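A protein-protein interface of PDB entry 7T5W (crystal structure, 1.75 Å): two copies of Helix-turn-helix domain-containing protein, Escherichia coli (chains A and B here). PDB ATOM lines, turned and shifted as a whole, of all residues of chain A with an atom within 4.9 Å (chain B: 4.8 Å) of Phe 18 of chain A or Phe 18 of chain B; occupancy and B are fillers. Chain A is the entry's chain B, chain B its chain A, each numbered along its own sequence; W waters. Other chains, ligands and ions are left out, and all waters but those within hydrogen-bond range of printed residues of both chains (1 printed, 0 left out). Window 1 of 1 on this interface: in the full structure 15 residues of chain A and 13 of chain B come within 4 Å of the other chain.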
ATOM      1  N   LEU A  14     -36.800 -20.547  13.717  1.00  0.00           N
ATOM      2  CA  LEU A  14     -35.420 -20.735  14.118  1.00  0.00           C
ATOM      3  C   LEU A  14     -34.656 -21.431  13.010  1.00  0.00           C
ATOM      4  O   LEU A  14     -33.548 -21.040  12.662  1.00  0.00           O
ATOM      5  CB  LEU A  14     -35.303 -21.559  15.393  1.00  0.00           C
ATOM      6  CG  LEU A  14     -35.630 -20.842  16.702  1.00  0.00           C
ATOM      7  CD1 LEU A  14     -35.961 -21.863  17.760  1.00  0.00           C
ATOM      8  CD2 LEU A  14     -34.443 -19.998  17.115  1.00  0.00           C
ATOM      9  N   ASP A  15     -35.261 -22.484  12.445  1.00  0.00           N
ATOM     10  CA  ASP A  15     -34.615 -23.182  11.344  1.00  0.00           C
ATOM     11  C   ASP A  15     -34.345 -22.251  10.175  1.00  0.00           C
ATOM     12  O   ASP A  15     -33.272 -22.300   9.555  1.00  0.00           O
ATOM     13  CB  ASP A  15     -35.506 -24.338  10.900  1.00  0.00           C
ATOM     14  CG  ASP A  15     -35.527 -25.473  11.915  1.00  0.00           C
ATOM     15  OD1 ASP A  15     -34.781 -25.394  12.926  1.00  0.00           O
ATOM     16  OD2 ASP A  15     -36.282 -26.453  11.688  1.00  0.00           O
ATOM     17  N   ASP A  16     -35.325 -21.431   9.820  1.00  0.00           N
ATOM     18  CA  ASP A  16     -35.149 -20.584   8.650  1.00  0.00           C
ATOM     19  C   ASP A  16     -34.044 -19.560   8.881  1.00  0.00           C
ATOM     20  O   ASP A  16     -33.305 -19.201   7.948  1.00  0.00           O
ATOM     21  CB  ASP A  16     -36.466 -19.901   8.292  1.00  0.00           C
ATOM     22  CG  ASP A  16     -37.504 -20.885   7.754  1.00  0.00           C
ATOM     23  OD1 ASP A  16     -37.085 -21.976   7.300  1.00  0.00           O
ATOM     24  OD2 ASP A  16     -38.716 -20.573   7.789  1.00  0.00           O
ATOM     25  N   ALA A  17     -33.933 -19.058  10.108  1.00  0.00           N
ATOM     26  CA  ALA A  17     -32.890 -18.077  10.407  1.00  0.00           C
ATOM     27  C   ALA A  17     -31.512 -18.736  10.392  1.00  0.00           C
ATOM     28  O   ALA A  17     -30.533 -18.116   9.964  1.00  0.00           O
ATOM     29  CB  ALA A  17     -33.169 -17.426  11.757  1.00  0.00           C
ATOM     30  N   PHE A  18     -31.428 -19.981  10.870  1.00  0.00           N
ATOM     31  CA  PHE A  18     -30.204 -20.778  10.738  1.00  0.00           C
ATOM     32  C   PHE A  18     -29.796 -20.875   9.281  1.00  0.00           C
ATOM     33  O   PHE A  18     -28.643 -20.600   8.928  1.00  0.00           O
ATOM     34  CB  PHE A  18     -30.448 -22.173  11.360  1.00  0.00           C
ATOM     35  CG  PHE A  18     -29.361 -23.179  11.101  1.00  0.00           C
ATOM     36  CD1 PHE A  18     -28.223 -23.191  11.886  1.00  0.00           C
ATOM     37  CD2 PHE A  18     -29.507 -24.169  10.148  1.00  0.00           C
ATOM     38  CE1 PHE A  18     -27.178 -24.102  11.664  1.00  0.00           C
ATOM     39  CE2 PHE A  18     -28.490 -25.095   9.915  1.00  0.00           C
ATOM     40  CZ  PHE A  18     -27.324 -25.088  10.716  1.00  0.00           C
ATOM     41  N   PHE A  19     -30.750 -21.198   8.398  1.00  0.00           N
ATOM     42  CA  PHE A  19     -30.374 -21.399   6.993  1.00  0.00           C
ATOM     43  C   PHE A  19     -29.972 -20.083   6.341  1.00  0.00           C
ATOM     44  O   PHE A  19     -29.055 -20.063   5.511  1.00  0.00           O
ATOM     45  CB  PHE A  19     -31.516 -22.093   6.252  1.00  0.00           C
ATOM     46  CG  PHE A  19     -31.156 -22.627   4.873  1.00  0.00           C
ATOM     47  CD1 PHE A  19     -29.967 -23.307   4.635  1.00  0.00           C
ATOM     48  CD2 PHE A  19     -32.044 -22.466   3.799  1.00  0.00           C
ATOM     49  CE1 PHE A  19     -29.646 -23.803   3.362  1.00  0.00           C
ATOM     50  CE2 PHE A  19     -31.729 -22.982   2.523  1.00  0.00           C
ATOM     51  CZ  PHE A  19     -30.514 -23.647   2.312  1.00  0.00           C
ATOM     52  N   ARG A  20     -30.626 -18.970   6.708  1.00  0.00           N
ATOM     53  CA  ARG A  20     -30.213 -17.677   6.166  1.00  0.00           C
ATOM     54  C   ARG A  20     -28.843 -17.271   6.691  1.00  0.00           C
ATOM     55  O   ARG A  20     -28.056 -16.656   5.956  1.00  0.00           O
ATOM     56  CB  ARG A  20     -31.243 -16.595   6.497  1.00  0.00           C
ATOM     57  CG  ARG A  20     -32.487 -16.613   5.611  1.00  0.00           C
ATOM     58  CD  ARG A  20     -33.306 -15.321   5.801  1.00  0.00           C
ATOM     59  NE  ARG A  20     -33.491 -15.035   7.221  1.00  0.00           N
ATOM     60  CZ  ARG A  20     -34.467 -15.542   7.959  1.00  0.00           C
ATOM     61  NH1 ARG A  20     -35.430 -16.278   7.422  1.00  0.00           N
ATOM     62  NH2 ARG A  20     -34.487 -15.296   9.265  1.00  0.00           N
ATOM     63  N   GLY A  21     -28.520 -17.640   7.927  1.00  0.00           N
ATOM     64  CA  GLY A  21     -27.193 -17.352   8.449  1.00  0.00           C
ATOM     65  C   GLY A  21     -26.112 -18.137   7.731  1.00  0.00           C
ATOM     66  O   GLY A  21     -25.030 -17.618   7.455  1.00  0.00           O
ATOM     67  N   TYR A  22     -26.404 -19.392   7.424  1.00  0.00           N
ATOM     68  CA  TYR A  22     -25.479 -20.213   6.645  1.00  0.00           C
ATOM     69  C   TYR A  22     -25.244 -19.634   5.266  1.00  0.00           C
ATOM     70  O   TYR A  22     -24.101 -19.568   4.778  1.00  0.00           O
ATOM     71  CB  TYR A  22     -26.037 -21.628   6.585  1.00  0.00           C
ATOM     72  CG  TYR A  22     -25.436 -22.536   5.550  1.00  0.00           C
ATOM     73  CD1 TYR A  22     -24.258 -23.199   5.777  1.00  0.00           C
ATOM     74  CD2 TYR A  22     -26.112 -22.761   4.364  1.00  0.00           C
ATOM     75  CE1 TYR A  22     -23.725 -24.065   4.811  1.00  0.00           C
ATOM     76  CE2 TYR A  22     -25.621 -23.588   3.413  1.00  0.00           C
ATOM     77  CZ  TYR A  22     -24.420 -24.215   3.612  1.00  0.00           C
ATOM     78  OH  TYR A  22     -23.925 -25.071   2.661  1.00  0.00           O
ATOM     79  N   LEU A  33     -18.878 -25.791   7.792  1.00  0.00           N
ATOM     80  CA  LEU A  33     -20.119 -26.151   8.484  1.00  0.00           C
ATOM     81  C   LEU A  33     -20.736 -27.424   7.918  1.00  0.00           C
ATOM     82  O   LEU A  33     -21.331 -28.225   8.657  1.00  0.00           O
ATOM     83  CB  LEU A  33     -21.130 -25.014   8.401  1.00  0.00           C
ATOM     84  CG  LEU A  33     -21.078 -24.057   9.581  1.00  0.00           C
ATOM     85  CD1 LEU A  33     -22.084 -22.953   9.384  1.00  0.00           C
ATOM     86  CD2 LEU A  33     -21.403 -24.781  10.913  1.00  0.00           C
ATOM     87  N   ARG A  34     -20.646 -27.631   6.604  1.00  0.00           N
ATOM     88  CA  ARG A  34     -21.092 -28.902   6.045  1.00  0.00           C
ATOM     89  C   ARG A  34     -20.300 -30.060   6.634  1.00  0.00           C
ATOM     90  O   ARG A  34     -20.864 -31.102   6.986  1.00  0.00           O
ATOM     91  CB  ARG A  34     -20.956 -28.886   4.509  1.00  0.00           C
ATOM     92  CG  ARG A  34     -21.936 -27.920   3.872  1.00  0.00           C
ATOM     93  CD  ARG A  34     -22.098 -28.113   2.401  1.00  0.00           C
ATOM     94  NE  ARG A  34     -20.882 -27.765   1.656  1.00  0.00           N
ATOM     95  CZ  ARG A  34     -20.623 -26.575   1.127  1.00  0.00           C
ATOM     96  NH1 ARG A  34     -21.493 -25.573   1.199  1.00  0.00           N
ATOM     97  NH2 ARG A  34     -19.473 -26.384   0.475  1.00  0.00           N
ATOM     98  N   LEU A  37     -21.611 -30.588  10.152  1.00  0.00           N
ATOM     99  CA  LEU A  37     -22.905 -31.263  10.128  1.00  0.00           C
ATOM    100  C   LEU A  37     -22.756 -32.761   9.894  1.00  0.00           C
ATOM    101  O   LEU A  37     -23.438 -33.574  10.517  1.00  0.00           O
ATOM    102  CB  LEU A  37     -23.802 -30.657   9.038  1.00  0.00           C
ATOM    103  CG  LEU A  37     -25.042 -31.469   8.699  1.00  0.00           C
ATOM    104  CD1 LEU A  37     -25.911 -31.420   9.947  1.00  0.00           C
ATOM    105  CD2 LEU A  37     -25.815 -30.944   7.482  1.00  0.00           C
ATOM    106  N   LEU B  14     -25.478 -28.558  -2.567  1.00  0.00           N
ATOM    107  CA  LEU B  14     -24.803 -28.686  -1.267  1.00  0.00           C
ATOM    108  C   LEU B  14     -25.554 -27.901  -0.196  1.00  0.00           C
ATOM    109  O   LEU B  14     -25.685 -28.354   0.946  1.00  0.00           O
ATOM    110  CB  LEU B  14     -23.367 -28.189  -1.355  1.00  0.00           C
ATOM    111  CG  LEU B  14     -22.408 -29.086  -2.137  1.00  0.00           C
ATOM    112  CD1 LEU B  14     -21.100 -28.375  -2.395  1.00  0.00           C
ATOM    113  CD2 LEU B  14     -22.165 -30.364  -1.357  1.00  0.00           C
ATOM    114  N   ASP B  15     -26.039 -26.720  -0.556  1.00  0.00           N
ATOM    115  CA  ASP B  15     -26.812 -25.929   0.402  1.00  0.00           C
ATOM    116  C   ASP B  15     -28.097 -26.647   0.780  1.00  0.00           C
ATOM    117  O   ASP B  15     -28.482 -26.683   1.967  1.00  0.00           O
ATOM    118  CB  ASP B  15     -27.093 -24.552  -0.185  1.00  0.00           C
ATOM    119  CG  ASP B  15     -25.855 -23.689  -0.240  1.00  0.00           C
ATOM    120  OD1 ASP B  15     -24.777 -24.133   0.221  1.00  0.00           O
ATOM    121  OD2 ASP B  15     -25.958 -22.560  -0.737  1.00  0.00           O
ATOM    122  N   ASP B  16     -28.784 -27.236  -0.207  1.00  0.00           N
ATOM    123  CA  ASP B  16     -30.030 -27.950   0.095  1.00  0.00           C
ATOM    124  C   ASP B  16     -29.760 -29.226   0.887  1.00  0.00           C
ATOM    125  O   ASP B  16     -30.542 -29.590   1.770  1.00  0.00           O
ATOM    126  CB  ASP B  16     -30.777 -28.290  -1.183  1.00  0.00           C
ATOM    127  CG  ASP B  16     -31.447 -27.070  -1.822  1.00  0.00           C
ATOM    128  OD1 ASP B  16     -31.501 -25.989  -1.199  1.00  0.00           O
ATOM    129  OD2 ASP B  16     -31.884 -27.214  -2.977  1.00  0.00           O
ATOM    130  N   ALA B  17     -28.656 -29.926   0.575  1.00  0.00           N
ATOM    131  CA  ALA B  17     -28.301 -31.117   1.344  1.00  0.00           C
ATOM    132  C   ALA B  17     -28.000 -30.738   2.784  1.00  0.00           C
ATOM    133  O   ALA B  17     -28.366 -31.457   3.724  1.00  0.00           O
ATOM    134  CB  ALA B  17     -27.085 -31.820   0.718  1.00  0.00           C
ATOM    135  N   PHE B  18     -27.324 -29.600   2.973  1.00  0.00           N
ATOM    136  CA  PHE B  18     -27.039 -29.113   4.315  1.00  0.00           C
ATOM    137  C   PHE B  18     -28.330 -28.870   5.082  1.00  0.00           C
ATOM    138  O   PHE B  18     -28.473 -29.307   6.220  1.00  0.00           O
ATOM    139  CB  PHE B  18     -26.238 -27.835   4.218  1.00  0.00           C
ATOM    140  CG  PHE B  18     -25.897 -27.205   5.531  1.00  0.00           C
ATOM    141  CD1 PHE B  18     -24.889 -27.701   6.311  1.00  0.00           C
ATOM    142  CD2 PHE B  18     -26.562 -26.062   5.943  1.00  0.00           C
ATOM    143  CE1 PHE B  18     -24.525 -27.084   7.531  1.00  0.00           C
ATOM    144  CE2 PHE B  18     -26.242 -25.450   7.141  1.00  0.00           C
ATOM    145  CZ  PHE B  18     -25.203 -25.956   7.940  1.00  0.00           C
ATOM    146  N   PHE B  19     -29.287 -28.188   4.451  1.00  0.00           N
ATOM    147  CA  PHE B  19     -30.502 -27.847   5.195  1.00  0.00           C
ATOM    148  C   PHE B  19     -31.325 -29.095   5.480  1.00  0.00           C
ATOM    149  O   PHE B  19     -31.901 -29.216   6.572  1.00  0.00           O
ATOM    150  CB  PHE B  19     -31.325 -26.830   4.434  1.00  0.00           C
ATOM    151  CG  PHE B  19     -32.326 -26.088   5.319  1.00  0.00           C
ATOM    152  CD1 PHE B  19     -32.098 -25.900   6.685  1.00  0.00           C
ATOM    153  CD2 PHE B  19     -33.458 -25.589   4.768  1.00  0.00           C
ATOM    154  CE1 PHE B  19     -33.035 -25.224   7.483  1.00  0.00           C
ATOM    155  CE2 PHE B  19     -34.374 -24.886   5.549  1.00  0.00           C
ATOM    156  CZ  PHE B  19     -34.148 -24.718   6.894  1.00  0.00           C
ATOM    157  N   ARG B  20     -31.428 -30.007   4.515  1.00  0.00           N
ATOM    158  CA  ARG B  20     -32.106 -31.284   4.735  1.00  0.00           C
ATOM    159  C   ARG B  20     -31.467 -32.048   5.885  1.00  0.00           C
ATOM    160  O   ARG B  20     -32.156 -32.609   6.761  1.00  0.00           O
ATOM    161  CB  ARG B  20     -32.021 -32.169   3.483  1.00  0.00           C
ATOM    162  CG  ARG B  20     -32.919 -31.815   2.327  1.00  0.00           C
ATOM    163  CD  ARG B  20     -33.010 -32.974   1.298  1.00  0.00           C
ATOM    164  NE  ARG B  20     -31.727 -33.430   0.764  1.00  0.00           N
ATOM    165  CZ  ARG B  20     -31.099 -32.885  -0.275  1.00  0.00           C
ATOM    166  NH1 ARG B  20     -31.553 -31.781  -0.856  1.00  0.00           N
ATOM    167  NH2 ARG B  20     -29.993 -33.458  -0.744  1.00  0.00           N
ATOM    168  N   GLY B  21     -30.138 -32.153   5.871  1.00  0.00           N
ATOM    169  CA  GLY B  21     -29.471 -32.871   6.926  1.00  0.00           C
ATOM    170  C   GLY B  21     -29.706 -32.245   8.289  1.00  0.00           C
ATOM    171  O   GLY B  21     -29.934 -32.945   9.276  1.00  0.00           O
ATOM    172  N   TYR B  22     -29.621 -30.922   8.364  1.00  0.00           N
ATOM    173  CA  TYR B  22     -29.916 -30.246   9.618  1.00  0.00           C
ATOM    174  C   TYR B  22     -31.332 -30.542  10.099  1.00  0.00           C
ATOM    175  O   TYR B  22     -31.556 -30.758  11.301  1.00  0.00           O
ATOM    176  CB  TYR B  22     -29.711 -28.737   9.427  1.00  0.00           C
ATOM    177  CG  TYR B  22     -30.343 -27.873  10.480  1.00  0.00           C
ATOM    178  CD1 TYR B  22     -29.700 -27.650  11.689  1.00  0.00           C
ATOM    179  CD2 TYR B  22     -31.538 -27.245  10.237  1.00  0.00           C
ATOM    180  CE1 TYR B  22     -30.261 -26.847  12.658  1.00  0.00           C
ATOM    181  CE2 TYR B  22     -32.118 -26.424  11.194  1.00  0.00           C
ATOM    182  CZ  TYR B  22     -31.483 -26.240  12.398  1.00  0.00           C
ATOM    183  OH  TYR B  22     -32.089 -25.423  13.329  1.00  0.00           O
ATOM    184  N   LEU B  33     -25.947 -27.362  16.454  1.00  0.00           N
ATOM    185  CA  LEU B  33     -25.475 -26.820  15.183  1.00  0.00           C
ATOM    186  C   LEU B  33     -25.774 -25.326  15.064  1.00  0.00           C
ATOM    187  O   LEU B  33     -24.967 -24.568  14.506  1.00  0.00           O
ATOM    188  CB  LEU B  33     -26.067 -27.608  14.026  1.00  0.00           C
ATOM    189  CG  LEU B  33     -25.181 -27.606  12.765  1.00  0.00           C
ATOM    190  CD1 LEU B  33     -23.762 -28.118  12.918  1.00  0.00           C
ATOM    191  CD2 LEU B  33     -25.879 -28.381  11.653  1.00  0.00           C
ATOM    192  N   ARG B  34     -26.903 -24.860  15.583  1.00  0.00           N
ATOM    193  CA  ARG B  34     -27.155 -23.420  15.554  1.00  0.00           C
ATOM    194  C   ARG B  34     -26.083 -22.656  16.345  1.00  0.00           C
ATOM    195  O   ARG B  34     -25.616 -21.588  15.919  1.00  0.00           O
ATOM    196  CB  ARG B  34     -28.543 -23.116  16.110  1.00  0.00           C
ATOM    197  CG  ARG B  34     -29.665 -23.601  15.179  1.00  0.00           C
ATOM    198  CD  ARG B  34     -31.022 -23.004  15.527  1.00  0.00           C
ATOM    199  NE  ARG B  34     -31.468 -23.365  16.861  1.00  0.00           N
ATOM    200  CZ  ARG B  34     -32.198 -24.432  17.146  1.00  0.00           C
ATOM    201  NH1 ARG B  34     -32.561 -25.287  16.211  1.00  0.00           N
ATOM    202  NH2 ARG B  34     -32.565 -24.654  18.413  1.00  0.00           N
ATOM    203  N   LEU B  37     -22.929 -22.561  14.316  1.00  0.00           N
ATOM    204  CA  LEU B  37     -22.992 -21.564  13.243  1.00  0.00           C
ATOM    205  C   LEU B  37     -22.691 -20.178  13.794  1.00  0.00           C
ATOM    206  O   LEU B  37     -21.969 -19.394  13.168  1.00  0.00           O
ATOM    207  CB  LEU B  37     -24.367 -21.576  12.550  1.00  0.00           C
ATOM    208  CG  LEU B  37     -24.829 -20.328  11.759  1.00  0.00           C
ATOM    209  CD1 LEU B  37     -24.019 -20.116  10.516  1.00  0.00           C
ATOM    210  CD2 LEU B  37     -26.321 -20.418  11.335  1.00  0.00           C
HETATM  211  O   HOH W   1     -22.003 -23.818  -1.053  1.00  0.00           O
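Phe 18 of chain A touches Leu 33 of chain B, and with the chains exchanged Leu 33 of chain A touches Phe 18 of chain B.
Phe 18 of chain A touches Arg 34 of chain B, and with the chains exchanged Arg 34 of chain A touches Phe 18 of chain B.
Tyr 22 of chain A touches Leu 37 of chain B, and with the chains exchanged Leu 37 of chain A touches Tyr 22 of chain B.
Arg 34 of chain A touches Leu 14 of chain B, but with the chains exchanged Leu 14 of chain A does not touch Arg 34 of chain B (4.3 Å).
Positions printed for both chains: 14, 15, 16, 17, 18, 19, 20, 21, 22, 33, 34 and 37.
The side-chain hydroxyl of Tyr 22 of chain B is in hydrogen-bond range of the guanidinium group of Arg 34 of chain B (2.9 Å).
OH of Tyr 22 of chain A sits at hydrogen-bond distance from NH1 of Arg 34 of chain A (2.9 Å).
Phe 18 of chain B touches Phe 18 of chain A (CE2 to CE2, 3.6 Å).
Tyr 22 of chain B touches Phe 18 of chain A (CD1 to CE2, 3.3 Å).
Phe 18 of chain A touches Arg 34 of chain B.
Phe 19 of chain A touches Asp 15 of chain B (CE1 to O, 3.4 Å).
CD2 of Phe 19 of chain A touches CD2 of Phe 19 of chain B (3.6 Å).
Tyr 22 of chain A touches Leu 37 of chain B.
Phe 18 of chain B touches Leu 33 of chain A.
CD1 of Leu 33 of chain A touches CD1 of Leu 37 of chain B (3.6 Å).
Leu 37 of chain A touches Phe 18 of chain B (CD2 to O, 3.4 Å).
Tyr 22 of chain B touches Leu 37 of chain A.
The side-chain hydroxyl of Tyr 22 of chain A lies within hydrogen-bond range of the side-chain carboxylate of Asp 15 of chain B, at 2.7 Å.
The guanidinium group (NH1) of Arg 34 of chain A lies within salt-bridge range of the side-chain carboxylate (OD1) of Asp 15 of chain B (3.7 Å).
The side-chain hydroxyl (OH) of Tyr 22 of chain B lies within hydrogen-bond range of the side-chain carboxylate (OD1) of Asp 15 of chain A (2.7 Å).
The side-chain carboxylate (OD1) of Asp 15 of chain A lies within salt-bridge range of the guanidinium group (NH1) of Arg 34 of chain B (3.97 Å).
Hydrophobic or aromatic side chains of chain B within 4 Å of the printed part of chain A: Leu 14, Phe 18, Phe 19, Tyr 22, Leu 33 and Leu 37.
Of the 12 printed residues of chain A, 7 touch a printed residue of chain B.
Phe 18 of chain A touches five residues of chain B.
Of chain A, only Phe 18, Tyr 22, Leu 33, Arg 34 and Leu 37 come within 4 Å of Phe 18 of chain B.
Of the printed residues of chain A, Tyr 22 of chain B touches Asp 15 (2.7 Å), Phe 18 (3.3 Å) and Leu 37 (3.9 Å).
Of the printed residues of chain B, Phe 19 of chain A touches Asp 15 (3.4 Å) and Phe 19 (3.6 Å).
Arg 20 of chain B touches none of the printed residues of chain A.
The nearest residue of chain B that does not touch Phe 18 of chain A is Phe 19 of chain B (4.5 Å).
The nearest printed residue of chain A that does not touch Asp 15 of chain B is Leu 37 of chain A (7.5 Å).
Water W1 lies within hydrogen-bond range of the guanidinium group (NH1) of Arg 34 of chain A (2.9 Å) and the side-chain carboxylate (OD1) of Asp 15 of chain B (3.1 Å).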
